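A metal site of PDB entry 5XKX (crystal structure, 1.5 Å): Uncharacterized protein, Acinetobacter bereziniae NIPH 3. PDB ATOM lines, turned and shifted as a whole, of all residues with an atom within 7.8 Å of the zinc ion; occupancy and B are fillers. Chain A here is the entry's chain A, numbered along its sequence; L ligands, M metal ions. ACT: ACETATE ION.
His 263 touches the zinc ion (NE2 to ZN, 3.6 Å).
OE1 of Glu 269 lies within salt-bridge range of NE of Arg 361 (2.8 Å). The backbone carbonyl oxygen (O) of Glu 269 sits at hydrogen-bond distance from the backbone NH (N) of Phe 332 (2.7 Å). NE1 of Trp 359 is in hydrogen-bond range of OE1 of Glu 269 (2.8 Å). A ring nitrogen (NE2) of His 265 sits close to the guanidinium group (NH2) of Arg 361. A ring nitrogen (ND1) of His 265 is in hydrogen-bond range of the backbone carbonyl oxygen of Pro 267, at 2.8 Å. N of His 263 sits at hydrogen-bond distance from O of His 338 (2.9 Å). The backbone carbonyl oxygen (O) of Ala 336 sits at hydrogen-bond distance from a ring nitrogen (ND1) of His 338 (2.8 Å). The side-chain hydroxyl (OH) of Tyr 260 lies close to a ring nitrogen (NE2) of His 263, at 3.4 Å.
The zinc ion is bound by OE2 of Glu 269 (1.9 Å), O of the ligand (1.9 Å), NE2 of His 265 (2.1 Å), NE2 of His 338 (2.1 Å) and OXT of the ligand (2.4 Å). The zinc ion has five donor atoms within binding distance.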
ATOM      1  N   TYR A 208      20.930  27.323 -15.565  1.00  0.00           N
ATOM      2  CA  TYR A 208      20.768  28.753 -15.364  1.00  0.00           C
ATOM      3  C   TYR A 208      20.779  29.167 -13.899  1.00  0.00           C
ATOM      4  O   TYR A 208      20.658  30.360 -13.617  1.00  0.00           O
ATOM      5  CB  TYR A 208      19.494  29.232 -16.044  1.00  0.00           C
ATOM      6  CG  TYR A 208      19.613  29.279 -17.544  1.00  0.00           C
ATOM      7  CD1 TYR A 208      20.686  29.946 -18.150  1.00  0.00           C
ATOM      8  CD2 TYR A 208      18.685  28.649 -18.355  1.00  0.00           C
ATOM      9  CE1 TYR A 208      20.799  30.001 -19.511  1.00  0.00           C
ATOM     10  CE2 TYR A 208      18.801  28.695 -19.738  1.00  0.00           C
ATOM     11  CZ  TYR A 208      19.865  29.369 -20.303  1.00  0.00           C
ATOM     12  OH  TYR A 208      19.986  29.428 -21.661  1.00  0.00           O
ATOM     13  N   TYR A 223      14.665  25.388 -14.190  1.00  0.00           N
ATOM     14  CA  TYR A 223      15.099  24.909 -15.485  1.00  0.00           C
ATOM     15  C   TYR A 223      16.166  23.822 -15.352  1.00  0.00           C
ATOM     16  O   TYR A 223      17.103  23.947 -14.560  1.00  0.00           O
ATOM     17  CB  TYR A 223      15.662  26.054 -16.343  1.00  0.00           C
ATOM     18  CG  TYR A 223      15.975  25.561 -17.727  1.00  0.00           C
ATOM     19  CD1 TYR A 223      14.958  25.310 -18.634  1.00  0.00           C
ATOM     20  CD2 TYR A 223      17.287  25.290 -18.107  1.00  0.00           C
ATOM     21  CE1 TYR A 223      15.230  24.832 -19.889  1.00  0.00           C
ATOM     22  CE2 TYR A 223      17.566  24.815 -19.382  1.00  0.00           C
ATOM     23  CZ  TYR A 223      16.531  24.577 -20.261  1.00  0.00           C
ATOM     24  OH  TYR A 223      16.783  24.112 -21.511  1.00  0.00           O
ATOM     25  N   TYR A 260      11.318  31.653 -20.250  1.00  0.00           N
ATOM     26  CA  TYR A 260      12.692  31.477 -20.710  1.00  0.00           C
ATOM     27  C   TYR A 260      12.962  32.648 -21.660  1.00  0.00           C
ATOM     28  O   TYR A 260      12.307  32.725 -22.713  1.00  0.00           O
ATOM     29  CB  TYR A 260      12.804  30.136 -21.431  1.00  0.00           C
ATOM     30  CG  TYR A 260      14.196  29.637 -21.800  1.00  0.00           C
ATOM     31  CD1 TYR A 260      15.274  30.505 -22.014  1.00  0.00           C
ATOM     32  CD2 TYR A 260      14.418  28.269 -21.989  1.00  0.00           C
ATOM     33  CE1 TYR A 260      16.525  30.017 -22.347  1.00  0.00           C
ATOM     34  CE2 TYR A 260      15.666  27.790 -22.322  1.00  0.00           C
ATOM     35  CZ  TYR A 260      16.717  28.657 -22.502  1.00  0.00           C
ATOM     36  OH  TYR A 260      17.946  28.169 -22.865  1.00  0.00           O
ATOM     37  N   HIS A 263      16.417  34.002 -26.672  1.00  0.00           N
ATOM     38  CA  HIS A 263      17.774  33.486 -26.756  1.00  0.00           C
ATOM     39  C   HIS A 263      18.037  32.948 -28.166  1.00  0.00           C
ATOM     40  O   HIS A 263      17.122  32.823 -28.982  1.00  0.00           O
ATOM     41  CB  HIS A 263      18.096  32.486 -25.628  1.00  0.00           C
ATOM     42  CG  HIS A 263      17.256  31.244 -25.630  1.00  0.00           C
ATOM     43  ND1 HIS A 263      15.921  31.238 -25.305  1.00  0.00           N
ATOM     44  CD2 HIS A 263      17.592  29.953 -25.861  1.00  0.00           C
ATOM     45  CE1 HIS A 263      15.453  30.007 -25.376  1.00  0.00           C
ATOM     46  NE2 HIS A 263      16.455  29.200 -25.692  1.00  0.00           N
ATOM     47  N   TYR A 264      19.308  32.668 -28.444  1.00  0.00           N
ATOM     48  CA  TYR A 264      19.729  32.349 -29.802  1.00  0.00           C
ATOM     49  C   TYR A 264      21.107  31.710 -29.694  1.00  0.00           C
ATOM     50  O   TYR A 264      21.761  31.777 -28.660  1.00  0.00           O
ATOM     51  CB  TYR A 264      19.760  33.606 -30.682  1.00  0.00           C
ATOM     52  CG  TYR A 264      20.703  34.642 -30.129  1.00  0.00           C
ATOM     53  CD1 TYR A 264      20.299  35.479 -29.096  1.00  0.00           C
ATOM     54  CD2 TYR A 264      22.014  34.747 -30.585  1.00  0.00           C
ATOM     55  CE1 TYR A 264      21.163  36.411 -28.546  1.00  0.00           C
ATOM     56  CE2 TYR A 264      22.881  35.680 -30.045  1.00  0.00           C
ATOM     57  CZ  TYR A 264      22.447  36.514 -29.023  1.00  0.00           C
ATOM     58  OH  TYR A 264      23.303  37.431 -28.468  1.00  0.00           O
ATOM     59  N   HIS A 265      21.519  31.055 -30.779  1.00  0.00           N
ATOM     60  CA  HIS A 265      22.823  30.391 -30.800  1.00  0.00           C
ATOM     61  C   HIS A 265      23.097  29.903 -32.208  1.00  0.00           C
ATOM     62  O   HIS A 265      22.175  29.741 -33.022  1.00  0.00           O
ATOM     63  CB  HIS A 265      22.888  29.214 -29.817  1.00  0.00           C
ATOM     64  CG  HIS A 265      21.620  28.421 -29.767  1.00  0.00           C
ATOM     65  ND1 HIS A 265      21.267  27.533 -30.760  1.00  0.00           N
ATOM     66  CD2 HIS A 265      20.607  28.413 -28.874  1.00  0.00           C
ATOM     67  CE1 HIS A 265      20.092  27.006 -30.479  1.00  0.00           C
ATOM     68  NE2 HIS A 265      19.658  27.529 -29.338  1.00  0.00           N
ATOM     69  N   PRO A 267      24.204  26.720 -33.222  1.00  0.00           N
ATOM     70  CA  PRO A 267      23.712  25.401 -33.629  1.00  0.00           C
ATOM     71  C   PRO A 267      22.211  25.394 -33.871  1.00  0.00           C
ATOM     72  O   PRO A 267      21.426  26.005 -33.133  1.00  0.00           O
ATOM     73  CB  PRO A 267      24.101  24.488 -32.450  1.00  0.00           C
ATOM     74  CG  PRO A 267      24.367  25.411 -31.300  1.00  0.00           C
ATOM     75  CD  PRO A 267      24.929  26.655 -31.937  1.00  0.00           C
ATOM     76  N   GLN A 268      21.835  24.706 -34.945  1.00  0.00           N
ATOM     77  CA  GLN A 268      20.438  24.418 -35.198  1.00  0.00           C
ATOM     78  C   GLN A 268      19.943  23.460 -34.132  1.00  0.00           C
ATOM     79  O   GLN A 268      20.697  22.667 -33.555  1.00  0.00           O
ATOM     80  CB  GLN A 268      20.278  23.789 -36.583  1.00  0.00           C
ATOM     81  CG  GLN A 268      20.836  24.632 -37.722  1.00  0.00           C
ATOM     82  CD  GLN A 268      22.252  24.244 -38.128  1.00  0.00           C
ATOM     83  OE1 GLN A 268      23.147  24.061 -37.287  1.00  0.00           O
ATOM     84  NE2 GLN A 268      22.455  24.088 -39.439  1.00  0.00           N
ATOM     85  N   GLU A 269      18.638  23.513 -33.884  1.00  0.00           N
ATOM     86  CA  GLU A 269      18.100  22.879 -32.691  1.00  0.00           C
ATOM     87  C   GLU A 269      16.708  22.360 -33.004  1.00  0.00           C
ATOM     88  O   GLU A 269      15.974  22.930 -33.817  1.00  0.00           O
ATOM     89  CB  GLU A 269      18.067  23.904 -31.566  1.00  0.00           C
ATOM     90  CG  GLU A 269      17.679  23.385 -30.191  1.00  0.00           C
ATOM     91  CD  GLU A 269      18.008  24.427 -29.148  1.00  0.00           C
ATOM     92  OE1 GLU A 269      18.911  24.192 -28.323  1.00  0.00           O
ATOM     93  OE2 GLU A 269      17.406  25.514 -29.198  1.00  0.00           O
ATOM     94  N   ILE A 270      16.334  21.261 -32.328  1.00  0.00           N
ATOM     95  CA  ILE A 270      15.048  20.615 -32.528  1.00  0.00           C
ATOM     96  C   ILE A 270      14.406  20.396 -31.171  1.00  0.00           C
ATOM     97  O   ILE A 270      15.073  19.949 -30.231  1.00  0.00           O
ATOM     98  CB  ILE A 270      15.196  19.257 -33.259  1.00  0.00           C
ATOM     99  CG1 ILE A 270      15.966  19.415 -34.570  1.00  0.00           C
ATOM    100  CG2 ILE A 270      13.819  18.601 -33.483  1.00  0.00           C
ATOM    101  CD1 ILE A 270      16.418  18.092 -35.163  1.00  0.00           C
ATOM    102  N   TYR A 271      13.109  20.675 -31.074  1.00  0.00           N
ATOM    103  CA  TYR A 271      12.359  20.372 -29.868  1.00  0.00           C
ATOM    104  C   TYR A 271      11.152  19.531 -30.224  1.00  0.00           C
ATOM    105  O   TYR A 271      10.418  19.846 -31.168  1.00  0.00           O
ATOM    106  CB  TYR A 271      11.880  21.638 -29.154  1.00  0.00           C
ATOM    107  CG  TYR A 271      12.889  22.273 -28.237  1.00  0.00           C
ATOM    108  CD1 TYR A 271      12.953  21.904 -26.910  1.00  0.00           C
ATOM    109  CD2 TYR A 271      13.745  23.258 -28.694  1.00  0.00           C
ATOM    110  CE1 TYR A 271      13.856  22.510 -26.047  1.00  0.00           C
ATOM    111  CE2 TYR A 271      14.672  23.854 -27.846  1.00  0.00           C
ATOM    112  CZ  TYR A 271      14.711  23.484 -26.517  1.00  0.00           C
ATOM    113  OH  TYR A 271      15.583  24.065 -25.638  1.00  0.00           O
ATOM    114  N   PHE A 332      14.866  24.963 -35.276  1.00  0.00           N
ATOM    115  CA  PHE A 332      15.394  26.311 -35.196  1.00  0.00           C
ATOM    116  C   PHE A 332      16.613  26.428 -36.104  1.00  0.00           C
ATOM    117  O   PHE A 332      17.625  25.758 -35.865  1.00  0.00           O
ATOM    118  CB  PHE A 332      15.818  26.645 -33.768  1.00  0.00           C
ATOM    119  CG  PHE A 332      14.727  26.522 -32.740  1.00  0.00           C
ATOM    120  CD1 PHE A 332      13.393  26.418 -33.089  1.00  0.00           C
ATOM    121  CD2 PHE A 332      15.058  26.524 -31.391  1.00  0.00           C
ATOM    122  CE1 PHE A 332      12.417  26.318 -32.102  1.00  0.00           C
ATOM    123  CE2 PHE A 332      14.094  26.417 -30.422  1.00  0.00           C
ATOM    124  CZ  PHE A 332      12.767  26.306 -30.782  1.00  0.00           C
ATOM    125  N   ALA A 336      18.278  31.652 -34.951  1.00  0.00           N
ATOM    126  CA  ALA A 336      16.859  31.983 -34.825  1.00  0.00           C
ATOM    127  C   ALA A 336      16.550  32.366 -33.383  1.00  0.00           C
ATOM    128  O   ALA A 336      16.973  31.680 -32.444  1.00  0.00           O
ATOM    129  CB  ALA A 336      15.991  30.794 -35.248  1.00  0.00           C
ATOM    130  N   ILE A 337      15.837  33.477 -33.211  1.00  0.00           N
ATOM    131  CA  ILE A 337      15.468  33.942 -31.885  1.00  0.00           C
ATOM    132  C   ILE A 337      14.343  33.051 -31.380  1.00  0.00           C
ATOM    133  O   ILE A 337      13.385  32.784 -32.107  1.00  0.00           O
ATOM    134  CB  ILE A 337      15.005  35.406 -31.928  1.00  0.00           C
ATOM    135  CG1 ILE A 337      15.971  36.266 -32.744  1.00  0.00           C
ATOM    136  CG2 ILE A 337      14.804  35.940 -30.518  1.00  0.00           C
ATOM    137  CD1 ILE A 337      17.373  36.269 -32.247  1.00  0.00           C
ATOM    138  N   HIS A 338      14.452  32.592 -30.138  1.00  0.00           N
ATOM    139  CA  HIS A 338      13.414  31.720 -29.608  1.00  0.00           C
ATOM    140  C   HIS A 338      13.214  31.956 -28.121  1.00  0.00           C
ATOM    141  O   HIS A 338      14.041  32.571 -27.446  1.00  0.00           O
ATOM    142  CB  HIS A 338      13.616  30.233 -29.944  1.00  0.00           C
ATOM    143  CG  HIS A 338      14.980  29.709 -29.660  1.00  0.00           C
ATOM    144  ND1 HIS A 338      16.087  30.026 -30.423  1.00  0.00           N
ATOM    145  CD2 HIS A 338      15.419  28.820 -28.729  1.00  0.00           C
ATOM    146  CE1 HIS A 338      17.136  29.374 -29.963  1.00  0.00           C
ATOM    147  NE2 HIS A 338      16.755  28.638 -28.935  1.00  0.00           N
ATOM    148  N   ALA A 339      12.079  31.470 -27.624  1.00  0.00           N
ATOM    149  CA  ALA A 339      11.700  31.675 -26.239  1.00  0.00           C
ATOM    150  C   ALA A 339      10.628  30.665 -25.886  1.00  0.00           C
ATOM    151  O   ALA A 339       9.903  30.187 -26.748  1.00  0.00           O
ATOM    152  CB  ALA A 339      11.142  33.092 -26.044  1.00  0.00           C
ATOM    153  N   PHE A 340      10.566  30.324 -24.599  1.00  0.00           N
ATOM    154  CA  PHE A 340       9.574  29.374 -24.088  1.00  0.00           C
ATOM    155  C   PHE A 340       8.877  30.038 -22.911  1.00  0.00           C
ATOM    156  O   PHE A 340       9.541  30.408 -21.928  1.00  0.00           O
ATOM    157  CB  PHE A 340      10.235  28.060 -23.657  1.00  0.00           C
ATOM    158  CG  PHE A 340      10.923  27.348 -24.792  1.00  0.00           C
ATOM    159  CD1 PHE A 340      10.179  26.718 -25.774  1.00  0.00           C
ATOM    160  CD2 PHE A 340      12.313  27.346 -24.883  1.00  0.00           C
ATOM    161  CE1 PHE A 340      10.804  26.075 -26.812  1.00  0.00           C
ATOM    162  CE2 PHE A 340      12.940  26.705 -25.931  1.00  0.00           C
ATOM    163  CZ  PHE A 340      12.185  26.069 -26.907  1.00  0.00           C
ATOM    164  N   TRP A 359      14.965  17.102 -26.638  1.00  0.00           N
ATOM    165  CA  TRP A 359      15.719  18.226 -27.151  1.00  0.00           C
ATOM    166  C   TRP A 359      16.933  17.731 -27.929  1.00  0.00           C
ATOM    167  O   TRP A 359      17.527  16.696 -27.592  1.00  0.00           O
ATOM    168  CB  TRP A 359      16.162  19.145 -25.991  1.00  0.00           C
ATOM    169  CG  TRP A 359      17.369  19.998 -26.290  1.00  0.00           C
ATOM    170  CD1 TRP A 359      17.398  21.198 -26.944  1.00  0.00           C
ATOM    171  CD2 TRP A 359      18.725  19.702 -25.937  1.00  0.00           C
ATOM    172  NE1 TRP A 359      18.682  21.666 -27.034  1.00  0.00           N
ATOM    173  CE2 TRP A 359      19.524  20.760 -26.424  1.00  0.00           C
ATOM    174  CE3 TRP A 359      19.345  18.635 -25.273  1.00  0.00           C
ATOM    175  CZ2 TRP A 359      20.904  20.797 -26.241  1.00  0.00           C
ATOM    176  CZ3 TRP A 359      20.729  18.674 -25.100  1.00  0.00           C
ATOM    177  CH2 TRP A 359      21.494  19.748 -25.585  1.00  0.00           C
ATOM    178  N   ALA A 360      17.291  18.446 -28.990  1.00  0.00           N
ATOM    179  CA  ALA A 360      18.475  18.081 -29.735  1.00  0.00           C
ATOM    180  C   ALA A 360      19.079  19.289 -30.427  1.00  0.00           C
ATOM    181  O   ALA A 360      18.383  20.265 -30.714  1.00  0.00           O
ATOM    182  CB  ALA A 360      18.179  17.010 -30.793  1.00  0.00           C
ATOM    183  N   ARG A 361      20.376  19.210 -30.683  1.00  0.00           N
ATOM    184  CA  ARG A 361      21.045  20.073 -31.638  1.00  0.00           C
ATOM    185  C   ARG A 361      21.685  19.204 -32.710  1.00  0.00           C
ATOM    186  O   ARG A 361      21.979  18.026 -32.485  1.00  0.00           O
ATOM    187  CB  ARG A 361      22.062  20.989 -30.961  1.00  0.00           C
ATOM    188  CG  ARG A 361      21.405  21.982 -30.035  1.00  0.00           C
ATOM    189  CD  ARG A 361      22.407  22.769 -29.213  1.00  0.00           C
ATOM    190  NE  ARG A 361      21.732  23.842 -28.495  1.00  0.00           N
ATOM    191  CZ  ARG A 361      22.345  24.743 -27.751  1.00  0.00           C
ATOM    192  NH1 ARG A 361      23.663  24.718 -27.602  1.00  0.00           N
ATOM    193  NH2 ARG A 361      21.644  25.693 -27.139  1.00  0.00           N
ATOM    194  N   THR A 371      24.930  29.086 -25.707  1.00  0.00           N
ATOM    195  CA  THR A 371      23.548  29.546 -25.696  1.00  0.00           C
ATOM    196  C   THR A 371      23.566  31.017 -25.273  1.00  0.00           C
ATOM    197  O   THR A 371      23.939  31.337 -24.145  1.00  0.00           O
ATOM    198  CB  THR A 371      22.715  28.716 -24.730  1.00  0.00           C
ATOM    199  OG1 THR A 371      22.774  27.337 -25.131  1.00  0.00           O
ATOM    200  CG2 THR A 371      21.254  29.183 -24.736  1.00  0.00           C
ATOM    201  N   GLN A 372      23.210  31.900 -26.197  1.00  0.00           N
ATOM    202  CA  GLN A 372      23.293  33.335 -25.961  1.00  0.00           C
ATOM    203  C   GLN A 372      21.942  33.854 -25.519  1.00  0.00           C
ATOM    204  O   GLN A 372      20.899  33.468 -26.060  1.00  0.00           O
ATOM    205  CB  GLN A 372      23.716  34.048 -27.247  1.00  0.00           C
ATOM    206  CG  GLN A 372      24.939  33.480 -27.915  1.00  0.00           C
ATOM    207  CD  GLN A 372      26.224  33.970 -27.301  1.00  0.00           C
ATOM    208  OE1 GLN A 372      26.220  34.532 -26.203  1.00  0.00           O
ATOM    209  NE2 GLN A 372      27.333  33.780 -28.010  1.00  0.00           N
HETATM  210  C   ACT L   1      17.981  26.272 -25.907  1.00  0.00           C
HETATM  211  O   ACT L   1      18.813  27.035 -26.476  1.00  0.00           O
HETATM  212  OXT ACT L   1      16.799  26.462 -26.269  1.00  0.00           O
HETATM  213  CH3 ACT L   1      18.366  25.213 -24.885  1.00  0.00           C
HETATM  214 ZN    ZN M   1      17.971  27.078 -28.227  1.00  0.00          ZN
